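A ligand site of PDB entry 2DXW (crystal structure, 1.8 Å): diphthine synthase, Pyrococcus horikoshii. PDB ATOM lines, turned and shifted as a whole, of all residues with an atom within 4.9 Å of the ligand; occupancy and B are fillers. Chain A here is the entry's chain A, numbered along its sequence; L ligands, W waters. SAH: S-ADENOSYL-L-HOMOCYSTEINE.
A nitrogen (N) of the ligand is in hydrogen-bond range of the backbone carbonyl oxygen (O) of Val 90 (2.6 Å). The backbone carbonyl oxygen of His 234 sits at hydrogen-bond distance from an oxygen (O2') of the ligand (2.6 Å). N of Leu 166 sits at hydrogen-bond distance from O2' of the ligand (3.0 Å). An oxygen (O3') of the ligand lies within hydrogen-bond range of the backbone carbonyl oxygen (O) of Leu 166 (2.7 Å). The side-chain hydroxyl (OG) of Ser 115 is in hydrogen-bond range of an oxygen (O) of the ligand (2.7 Å). N of Ala 209 is in hydrogen-bond range of N1 of the ligand, at 2.9 Å. A nitrogen (N6) of the ligand is in hydrogen-bond range of the backbone carbonyl oxygen (O) of Ala 209, at 2.7 Å. An oxygen (O) of the ligand sits at hydrogen-bond distance from the backbone NH (N) of Asp 87 (2.9 Å). O of Asp 87 lies within hydrogen-bond range of N of the ligand, 2.8 Å away. N of Ile 116 lies within hydrogen-bond range of OXT of the ligand, at 3.0 Å. The side-chain hydroxyl of Ser 37 lies close to a nitrogen (N7) of the ligand, 3.5 Å away. The backbone carbonyl oxygen (O) of Leu 10 is in hydrogen-bond range of a nitrogen (N6) of the ligand, at 3.1 Å. The backbone NH (N) of Arg 208 lies within hydrogen-bond range of a nitrogen (N1) of the ligand.
OG of Ser 115 lies close to N of Tyr 117 (3.2 Å). N of Arg 208 lies within hydrogen-bond range of O of Pro 233. The backbone carbonyl oxygen (O) of Leu 206 lies within hydrogen-bond range of the backbone NH (N) of Ile 235, at 3.0 Å.
SD of the ligand sits close to O of Thr 36 (3.7 Å). Residues that only touch the ligand: Pro 233, Phe 165, Leu 206, Gly 86, Thr 92, Ala 91, Ile 235 and Pro 85. Hydrophobic or aromatic side chains that line the ligand: Leu 10, Val 90, Ala 91, Ile 116, Phe 165, Leu 166, Ala 209, Pro 233 and Ile 235. Within 4 Å of the ligand: Leu 10, Thr 36, Ser 37, Pro 85, Gly 86, Asp 87, Val 90, Ala 91, Thr 92, Ser 115, Ile 116, Phe 165, Leu 166, Leu 206, Arg 208, Ala 209, Pro 233, His 234 and Ile 235.
Water W4 lies within hydrogen-bond range of the side-chain hydroxyl (OG1) of Thr 36 (2.7 Å), a nitrogen (N) of the ligand (2.8 Å) and the backbone carbonyl oxygen (O) of Pro 85 (2.8 Å). Water W2 bridges an oxygen (O3') of the ligand (2.8 Å) and the backbone carbonyl oxygen (O) of Asp 167 (3.0 Å).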
ATOM      1  N   LEU A  10     -23.171   6.280  -9.491  1.00  0.00           N
ATOM      2  CA  LEU A  10     -23.799   7.601  -9.495  1.00  0.00           C
ATOM      3  C   LEU A  10     -23.056   8.906  -9.310  1.00  0.00           C
ATOM      4  O   LEU A  10     -23.309   9.868 -10.037  1.00  0.00           O
ATOM      5  CB  LEU A  10     -24.919   7.599  -8.453  1.00  0.00           C
ATOM      6  CG  LEU A  10     -25.984   6.495  -8.491  1.00  0.00           C
ATOM      7  CD1 LEU A  10     -26.693   6.437  -7.150  1.00  0.00           C
ATOM      8  CD2 LEU A  10     -26.964   6.763  -9.617  1.00  0.00           C
ATOM      9  N   TYR A  11     -22.147   8.956  -8.352  1.00  0.00           N
ATOM     10  CA  TYR A  11     -21.513  10.222  -8.016  1.00  0.00           C
ATOM     11  C   TYR A  11     -19.984  10.291  -7.942  1.00  0.00           C
ATOM     12  O   TYR A  11     -19.383  11.193  -8.533  1.00  0.00           O
ATOM     13  CB  TYR A  11     -22.126  10.684  -6.700  1.00  0.00           C
ATOM     14  CG  TYR A  11     -21.702  12.039  -6.194  1.00  0.00           C
ATOM     15  CD1 TYR A  11     -22.114  13.209  -6.851  1.00  0.00           C
ATOM     16  CD2 TYR A  11     -20.932  12.157  -5.049  1.00  0.00           C
ATOM     17  CE1 TYR A  11     -21.755  14.467  -6.350  1.00  0.00           C
ATOM     18  CE2 TYR A  11     -20.573  13.415  -4.548  1.00  0.00           C
ATOM     19  CZ  TYR A  11     -20.992  14.555  -5.198  1.00  0.00           C
ATOM     20  OH  TYR A  11     -20.643  15.789  -4.683  1.00  0.00           O
ATOM     21  N   THR A  36     -22.007   9.825 -21.367  1.00  0.00           N
ATOM     22  CA  THR A  36     -23.390   9.393 -21.157  1.00  0.00           C
ATOM     23  C   THR A  36     -23.984   9.963 -19.875  1.00  0.00           C
ATOM     24  O   THR A  36     -25.206  10.009 -19.714  1.00  0.00           O
ATOM     25  CB  THR A  36     -23.507   7.858 -21.120  1.00  0.00           C
ATOM     26  OG1 THR A  36     -22.650   7.328 -20.102  1.00  0.00           O
ATOM     27  CG2 THR A  36     -23.144   7.263 -22.457  1.00  0.00           C
ATOM     28  N   SER A  37     -23.132  10.380 -18.944  1.00  0.00           N
ATOM     29  CA  SER A  37     -23.607  10.954 -17.692  1.00  0.00           C
ATOM     30  C   SER A  37     -22.504  11.712 -16.986  1.00  0.00           C
ATOM     31  O   SER A  37     -21.343  11.670 -17.410  1.00  0.00           O
ATOM     32  CB  SER A  37     -24.145   9.850 -16.773  1.00  0.00           C
ATOM     33  OG  SER A  37     -24.808  10.424 -15.672  1.00  0.00           O
ATOM     34  N   LEU A  38     -22.864  12.410 -15.925  1.00  0.00           N
ATOM     35  CA  LEU A  38     -21.909  13.190 -15.144  1.00  0.00           C
ATOM     36  C   LEU A  38     -21.730  12.676 -13.733  1.00  0.00           C
ATOM     37  O   LEU A  38     -22.700  12.563 -12.967  1.00  0.00           O
ATOM     38  CB  LEU A  38     -22.354  14.662 -15.083  1.00  0.00           C
ATOM     39  CG  LEU A  38     -21.540  15.601 -14.193  1.00  0.00           C
ATOM     40  CD1 LEU A  38     -20.133  15.774 -14.740  1.00  0.00           C
ATOM     41  CD2 LEU A  38     -22.236  16.962 -14.113  1.00  0.00           C
ATOM     42  N   PRO A  85     -20.204   5.716 -16.451  1.00  0.00           N
ATOM     43  CA  PRO A  85     -20.866   6.262 -15.267  1.00  0.00           C
ATOM     44  C   PRO A  85     -22.127   5.429 -15.019  1.00  0.00           C
ATOM     45  O   PRO A  85     -22.632   4.803 -15.958  1.00  0.00           O
ATOM     46  CB  PRO A  85     -21.208   7.691 -15.688  1.00  0.00           C
ATOM     47  CG  PRO A  85     -20.143   8.022 -16.692  1.00  0.00           C
ATOM     48  CD  PRO A  85     -20.063   6.746 -17.492  1.00  0.00           C
ATOM     49  N   GLY A  86     -22.623   5.423 -13.788  1.00  0.00           N
ATOM     50  CA  GLY A  86     -23.815   4.667 -13.457  1.00  0.00           C
ATOM     51  C   GLY A  86     -23.714   3.204 -13.866  1.00  0.00           C
ATOM     52  O   GLY A  86     -22.673   2.587 -13.677  1.00  0.00           O
ATOM     53  N   ASP A  87     -24.801   2.657 -14.402  1.00  0.00           N
ATOM     54  CA  ASP A  87     -24.806   1.278 -14.879  1.00  0.00           C
ATOM     55  C   ASP A  87     -24.524   1.394 -16.371  1.00  0.00           C
ATOM     56  O   ASP A  87     -25.160   2.186 -17.072  1.00  0.00           O
ATOM     57  CB  ASP A  87     -26.168   0.626 -14.629  1.00  0.00           C
ATOM     58  CG  ASP A  87     -26.219  -0.808 -15.132  1.00  0.00           C
ATOM     59  OD1 ASP A  87     -26.166  -1.008 -16.360  1.00  0.00           O
ATOM     60  OD2 ASP A  87     -26.300  -1.729 -14.290  1.00  0.00           O
ATOM     61  N   VAL A  90     -27.778   1.188 -18.881  1.00  0.00           N
ATOM     62  CA  VAL A  90     -28.996   1.939 -18.596  1.00  0.00           C
ATOM     63  C   VAL A  90     -29.011   3.309 -19.280  1.00  0.00           C
ATOM     64  O   VAL A  90     -28.164   4.152 -19.003  1.00  0.00           O
ATOM     65  CB  VAL A  90     -29.186   2.148 -17.085  1.00  0.00           C
ATOM     66  CG1 VAL A  90     -30.384   3.054 -16.815  1.00  0.00           C
ATOM     67  CG2 VAL A  90     -29.394   0.807 -16.395  1.00  0.00           C
ATOM     68  N   ALA A  91     -29.969   3.531 -20.162  1.00  0.00           N
ATOM     69  CA  ALA A  91     -30.088   4.805 -20.862  1.00  0.00           C
ATOM     70  C   ALA A  91     -28.840   5.135 -21.674  1.00  0.00           C
ATOM     71  O   ALA A  91     -28.440   6.300 -21.797  1.00  0.00           O
ATOM     72  CB  ALA A  91     -30.377   5.928 -19.864  1.00  0.00           C
ATOM     73  N   THR A  92     -28.218   4.092 -22.215  1.00  0.00           N
ATOM     74  CA  THR A  92     -27.087   4.185 -23.107  1.00  0.00           C
ATOM     75  C   THR A  92     -27.372   3.239 -24.247  1.00  0.00           C
ATOM     76  O   THR A  92     -28.305   2.466 -24.202  1.00  0.00           O
ATOM     77  CB  THR A  92     -25.798   3.765 -22.383  1.00  0.00           C
ATOM     78  OG1 THR A  92     -25.762   2.345 -22.258  1.00  0.00           O
ATOM     79  CG2 THR A  92     -25.660   4.404 -21.007  1.00  0.00           C
ATOM     80  N   PRO A 114     -24.698   1.228  -9.186  1.00  0.00           N
ATOM     81  CA  PRO A 114     -25.894   2.019  -8.877  1.00  0.00           C
ATOM     82  C   PRO A 114     -26.281   2.874 -10.084  1.00  0.00           C
ATOM     83  O   PRO A 114     -25.424   3.515 -10.696  1.00  0.00           O
ATOM     84  CB  PRO A 114     -25.461   2.887  -7.692  1.00  0.00           C
ATOM     85  CG  PRO A 114     -24.392   2.088  -7.054  1.00  0.00           C
ATOM     86  CD  PRO A 114     -23.625   1.491  -8.200  1.00  0.00           C
ATOM     87  N   SER A 115     -27.572   2.867 -10.406  1.00  0.00           N
ATOM     88  CA  SER A 115     -28.097   3.610 -11.549  1.00  0.00           C
ATOM     89  C   SER A 115     -29.146   4.623 -11.098  1.00  0.00           C
ATOM     90  O   SER A 115     -29.888   4.377 -10.146  1.00  0.00           O
ATOM     91  CB  SER A 115     -28.732   2.634 -12.540  1.00  0.00           C
ATOM     92  OG  SER A 115     -29.401   3.323 -13.585  1.00  0.00           O
ATOM     93  N   ILE A 116     -29.233   5.753 -11.786  1.00  0.00           N
ATOM     94  CA  ILE A 116     -30.224   6.755 -11.420  1.00  0.00           C
ATOM     95  C   ILE A 116     -31.621   6.170 -11.586  1.00  0.00           C
ATOM     96  O   ILE A 116     -32.562   6.556 -10.872  1.00  0.00           O
ATOM     97  CB  ILE A 116     -30.085   8.023 -12.297  1.00  0.00           C
ATOM     98  CG1 ILE A 116     -30.984   9.129 -11.756  1.00  0.00           C
ATOM     99  CG2 ILE A 116     -30.453   7.697 -13.737  1.00  0.00           C
ATOM    100  CD1 ILE A 116     -30.634   9.551 -10.335  1.00  0.00           C
ATOM    101  N   TYR A 117     -31.772   5.232 -12.515  1.00  0.00           N
ATOM    102  CA  TYR A 117     -33.060   4.600 -12.789  1.00  0.00           C
ATOM    103  C   TYR A 117     -33.678   3.960 -11.540  1.00  0.00           C
ATOM    104  O   TYR A 117     -34.894   3.970 -11.373  1.00  0.00           O
ATOM    105  CB  TYR A 117     -32.885   3.554 -13.896  1.00  0.00           C
ATOM    106  CG  TYR A 117     -34.169   2.867 -14.354  1.00  0.00           C
ATOM    107  CD1 TYR A 117     -35.152   3.578 -15.038  1.00  0.00           C
ATOM    108  CD2 TYR A 117     -34.366   1.505 -14.136  1.00  0.00           C
ATOM    109  CE1 TYR A 117     -36.311   2.934 -15.496  1.00  0.00           C
ATOM    110  CE2 TYR A 117     -35.504   0.854 -14.590  1.00  0.00           C
ATOM    111  CZ  TYR A 117     -36.475   1.573 -15.272  1.00  0.00           C
ATOM    112  OH  TYR A 117     -37.598   0.924 -15.731  1.00  0.00           O
ATOM    113  N   PHE A 165     -34.997  11.762 -17.796  1.00  0.00           N
ATOM    114  CA  PHE A 165     -33.548  11.887 -17.866  1.00  0.00           C
ATOM    115  C   PHE A 165     -33.371  13.266 -18.490  1.00  0.00           C
ATOM    116  O   PHE A 165     -34.163  13.656 -19.334  1.00  0.00           O
ATOM    117  CB  PHE A 165     -32.968  10.828 -18.801  1.00  0.00           C
ATOM    118  CG  PHE A 165     -33.078   9.429 -18.291  1.00  0.00           C
ATOM    119  CD1 PHE A 165     -32.170   8.937 -17.360  1.00  0.00           C
ATOM    120  CD2 PHE A 165     -34.100   8.596 -18.735  1.00  0.00           C
ATOM    121  CE1 PHE A 165     -32.269   7.630 -16.876  1.00  0.00           C
ATOM    122  CE2 PHE A 165     -34.219   7.281 -18.258  1.00  0.00           C
ATOM    123  CZ  PHE A 165     -33.296   6.806 -17.330  1.00  0.00           C
ATOM    124  N   LEU A 166     -32.335  13.989 -18.077  1.00  0.00           N
ATOM    125  CA  LEU A 166     -32.094  15.325 -18.639  1.00  0.00           C
ATOM    126  C   LEU A 166     -30.891  15.300 -19.575  1.00  0.00           C
ATOM    127  O   LEU A 166     -29.947  14.519 -19.383  1.00  0.00           O
ATOM    128  CB  LEU A 166     -31.907  16.332 -17.512  1.00  0.00           C
ATOM    129  CG  LEU A 166     -33.083  16.385 -16.524  1.00  0.00           C
ATOM    130  CD1 LEU A 166     -32.905  17.566 -15.578  1.00  0.00           C
ATOM    131  CD2 LEU A 166     -34.404  16.507 -17.281  1.00  0.00           C
ATOM    132  N   ASP A 167     -30.931  16.138 -20.600  1.00  0.00           N
ATOM    133  CA  ASP A 167     -29.870  16.174 -21.606  1.00  0.00           C
ATOM    134  C   ASP A 167     -28.488  16.502 -21.074  1.00  0.00           C
ATOM    135  O   ASP A 167     -28.337  17.148 -20.030  1.00  0.00           O
ATOM    136  CB  ASP A 167     -30.241  17.158 -22.722  1.00  0.00           C
ATOM    137  CG  ASP A 167     -29.649  16.773 -24.072  1.00  0.00           C
ATOM    138  OD1 ASP A 167     -28.909  15.770 -24.132  1.00  0.00           O
ATOM    139  OD2 ASP A 167     -29.940  17.482 -25.063  1.00  0.00           O
ATOM    140  N   ILE A 168     -27.474  16.043 -21.794  1.00  0.00           N
ATOM    141  CA  ILE A 168     -26.091  16.294 -21.444  1.00  0.00           C
ATOM    142  C   ILE A 168     -25.255  16.419 -22.716  1.00  0.00           C
ATOM    143  O   ILE A 168     -25.423  15.641 -23.659  1.00  0.00           O
ATOM    144  CB  ILE A 168     -25.494  15.168 -20.559  1.00  0.00           C
ATOM    145  CG1 ILE A 168     -23.990  15.388 -20.367  1.00  0.00           C
ATOM    146  CG2 ILE A 168     -25.769  13.800 -21.190  1.00  0.00           C
ATOM    147  CD1 ILE A 168     -23.326  14.374 -19.445  1.00  0.00           C
ATOM    148  N   LEU A 206     -34.396  15.470  -8.176  1.00  0.00           N
ATOM    149  CA  LEU A 206     -33.346  14.733  -7.486  1.00  0.00           C
ATOM    150  C   LEU A 206     -32.048  15.165  -8.117  1.00  0.00           C
ATOM    151  O   LEU A 206     -31.832  14.969  -9.316  1.00  0.00           O
ATOM    152  CB  LEU A 206     -33.533  13.219  -7.644  1.00  0.00           C
ATOM    153  CG  LEU A 206     -32.418  12.353  -7.023  1.00  0.00           C
ATOM    154  CD1 LEU A 206     -32.271  12.672  -5.530  1.00  0.00           C
ATOM    155  CD2 LEU A 206     -32.734  10.875  -7.222  1.00  0.00           C
ATOM    156  N   ALA A 207     -31.174  15.779  -7.323  1.00  0.00           N
ATOM    157  CA  ALA A 207     -29.907  16.255  -7.836  1.00  0.00           C
ATOM    158  C   ALA A 207     -28.732  15.605  -7.109  1.00  0.00           C
ATOM    159  O   ALA A 207     -28.708  15.532  -5.892  1.00  0.00           O
ATOM    160  CB  ALA A 207     -29.827  17.769  -7.718  1.00  0.00           C
ATOM    161  N   ARG A 208     -27.773  15.127  -7.908  1.00  0.00           N
ATOM    162  CA  ARG A 208     -26.561  14.495  -7.406  1.00  0.00           C
ATOM    163  C   ARG A 208     -26.841  13.252  -6.553  1.00  0.00           C
ATOM    164  O   ARG A 208     -26.309  13.103  -5.440  1.00  0.00           O
ATOM    165  CB  ARG A 208     -25.719  15.511  -6.621  1.00  0.00           C
ATOM    166  CG  ARG A 208     -25.341  16.743  -7.459  1.00  0.00           C
ATOM    167  CD  ARG A 208     -24.556  17.765  -6.642  1.00  0.00           C
ATOM    168  NE  ARG A 208     -25.253  18.068  -5.393  1.00  0.00           N
ATOM    169  CZ  ARG A 208     -26.388  18.749  -5.302  1.00  0.00           C
ATOM    170  NH1 ARG A 208     -26.979  19.220  -6.391  1.00  0.00           N
ATOM    171  NH2 ARG A 208     -26.954  18.911  -4.113  1.00  0.00           N
ATOM    172  N   ALA A 209     -27.675  12.365  -7.077  1.00  0.00           N
ATOM    173  CA  ALA A 209     -27.971  11.117  -6.377  1.00  0.00           C
ATOM    174  C   ALA A 209     -26.619  10.432  -6.236  1.00  0.00           C
ATOM    175  O   ALA A 209     -25.745  10.575  -7.089  1.00  0.00           O
ATOM    176  CB  ALA A 209     -28.911  10.249  -7.219  1.00  0.00           C
ATOM    177  N   GLY A 210     -26.445   9.679  -5.151  1.00  0.00           N
ATOM    178  CA  GLY A 210     -25.168   9.006  -4.938  1.00  0.00           C
ATOM    179  C   GLY A 210     -24.323   9.731  -3.919  1.00  0.00           C
ATOM    180  O   GLY A 210     -23.551   9.129  -3.188  1.00  0.00           O
ATOM    181  N   PRO A 233     -25.382  16.482 -11.822  1.00  0.00           N
ATOM    182  CA  PRO A 233     -26.554  16.218 -12.668  1.00  0.00           C
ATOM    183  C   PRO A 233     -27.892  16.259 -11.921  1.00  0.00           C
ATOM    184  O   PRO A 233     -27.958  16.038 -10.711  1.00  0.00           O
ATOM    185  CB  PRO A 233     -26.260  14.834 -13.223  1.00  0.00           C
ATOM    186  CG  PRO A 233     -25.576  14.168 -12.056  1.00  0.00           C
ATOM    187  CD  PRO A 233     -24.634  15.244 -11.548  1.00  0.00           C
ATOM    188  N   HIS A 234     -28.948  16.533 -12.677  1.00  0.00           N
ATOM    189  CA  HIS A 234     -30.304  16.610 -12.147  1.00  0.00           C
ATOM    190  C   HIS A 234     -31.195  15.655 -12.928  1.00  0.00           C
ATOM    191  O   HIS A 234     -30.922  15.325 -14.080  1.00  0.00           O
ATOM    192  CB  HIS A 234     -30.922  18.004 -12.367  1.00  0.00           C
ATOM    193  CG  HIS A 234     -30.269  19.106 -11.601  1.00  0.00           C
ATOM    194  ND1 HIS A 234     -30.752  20.405 -11.638  1.00  0.00           N
ATOM    195  CD2 HIS A 234     -29.194  19.133 -10.795  1.00  0.00           C
ATOM    196  CE1 HIS A 234     -29.989  21.170 -10.883  1.00  0.00           C
ATOM    197  NE2 HIS A 234     -29.037  20.425 -10.351  1.00  0.00           N
ATOM    198  N   ILE A 235     -32.277  15.227 -12.291  1.00  0.00           N
ATOM    199  CA  ILE A 235     -33.262  14.413 -12.960  1.00  0.00           C
ATOM    200  C   ILE A 235     -34.597  14.992 -12.505  1.00  0.00           C
ATOM    201  O   ILE A 235     -34.723  15.477 -11.375  1.00  0.00           O
ATOM    202  CB  ILE A 235     -33.116  12.917 -12.597  1.00  0.00           C
ATOM    203  CG1 ILE A 235     -33.816  12.078 -13.658  1.00  0.00           C
ATOM    204  CG2 ILE A 235     -33.682  12.632 -11.219  1.00  0.00           C
ATOM    205  CD1 ILE A 235     -33.111  10.778 -13.973  1.00  0.00           C
HETATM  206  N   SAH L   1     -26.292   4.756 -17.332  1.00  0.00           N
HETATM  207  CA  SAH L   1     -26.597   5.961 -16.444  1.00  0.00           C
HETATM  208  CB  SAH L   1     -27.561   6.974 -16.989  1.00  0.00           C
HETATM  209  CG  SAH L   1     -27.251   7.645 -18.319  1.00  0.00           C
HETATM  210  SD  SAH L   1     -28.511   8.951 -18.573  1.00  0.00           S
HETATM  211  C   SAH L   1     -27.118   5.385 -15.068  1.00  0.00           C
HETATM  212  O   SAH L   1     -27.203   4.150 -14.929  1.00  0.00           O
HETATM  213  OXT SAH L   1     -27.412   6.256 -14.154  1.00  0.00           O
HETATM  214  C5' SAH L   1     -27.692  10.307 -17.812  1.00  0.00           C
HETATM  215  C4' SAH L   1     -28.732  11.285 -17.151  1.00  0.00           C
HETATM  216  O4' SAH L   1     -29.291  10.619 -15.989  1.00  0.00           O
HETATM  217  C3' SAH L   1     -28.174  12.576 -16.651  1.00  0.00           C
HETATM  218  O3' SAH L   1     -28.148  13.549 -17.689  1.00  0.00           O
HETATM  219  C2' SAH L   1     -29.121  12.899 -15.479  1.00  0.00           C
HETATM  220  O2' SAH L   1     -30.325  13.522 -15.924  1.00  0.00           O
HETATM  221  C1' SAH L   1     -29.352  11.532 -14.811  1.00  0.00           C
HETATM  222  N9  SAH L   1     -28.423  11.178 -13.881  1.00  0.00           N
HETATM  223  C8  SAH L   1     -27.313  10.352 -13.879  1.00  0.00           C
HETATM  224  N7  SAH L   1     -26.671  10.280 -12.759  1.00  0.00           N
HETATM  225  C5  SAH L   1     -27.406  11.132 -11.880  1.00  0.00           C
HETATM  226  C6  SAH L   1     -27.202  11.472 -10.502  1.00  0.00           C
HETATM  227  N6  SAH L   1     -26.208  10.994  -9.744  1.00  0.00           N
HETATM  228  N1  SAH L   1     -28.138  12.351  -9.981  1.00  0.00           N
HETATM  229  C2  SAH L   1     -29.166  12.864 -10.702  1.00  0.00           C
HETATM  230  N3  SAH L   1     -29.389  12.558 -12.034  1.00  0.00           N
HETATM  231  C4  SAH L   1     -28.470  11.692 -12.548  1.00  0.00           C
HETATM  232  O   HOH W   1     -25.283   7.755 -12.897  1.00  0.00           O
HETATM  233  O   HOH W   2     -27.072  16.160 -17.469  1.00  0.00           O
HETATM  234  O   HOH W   3     -23.409   9.341 -13.397  1.00  0.00           O
HETATM  235  O   HOH W   4     -23.991   6.042 -18.120  1.00  0.00           O
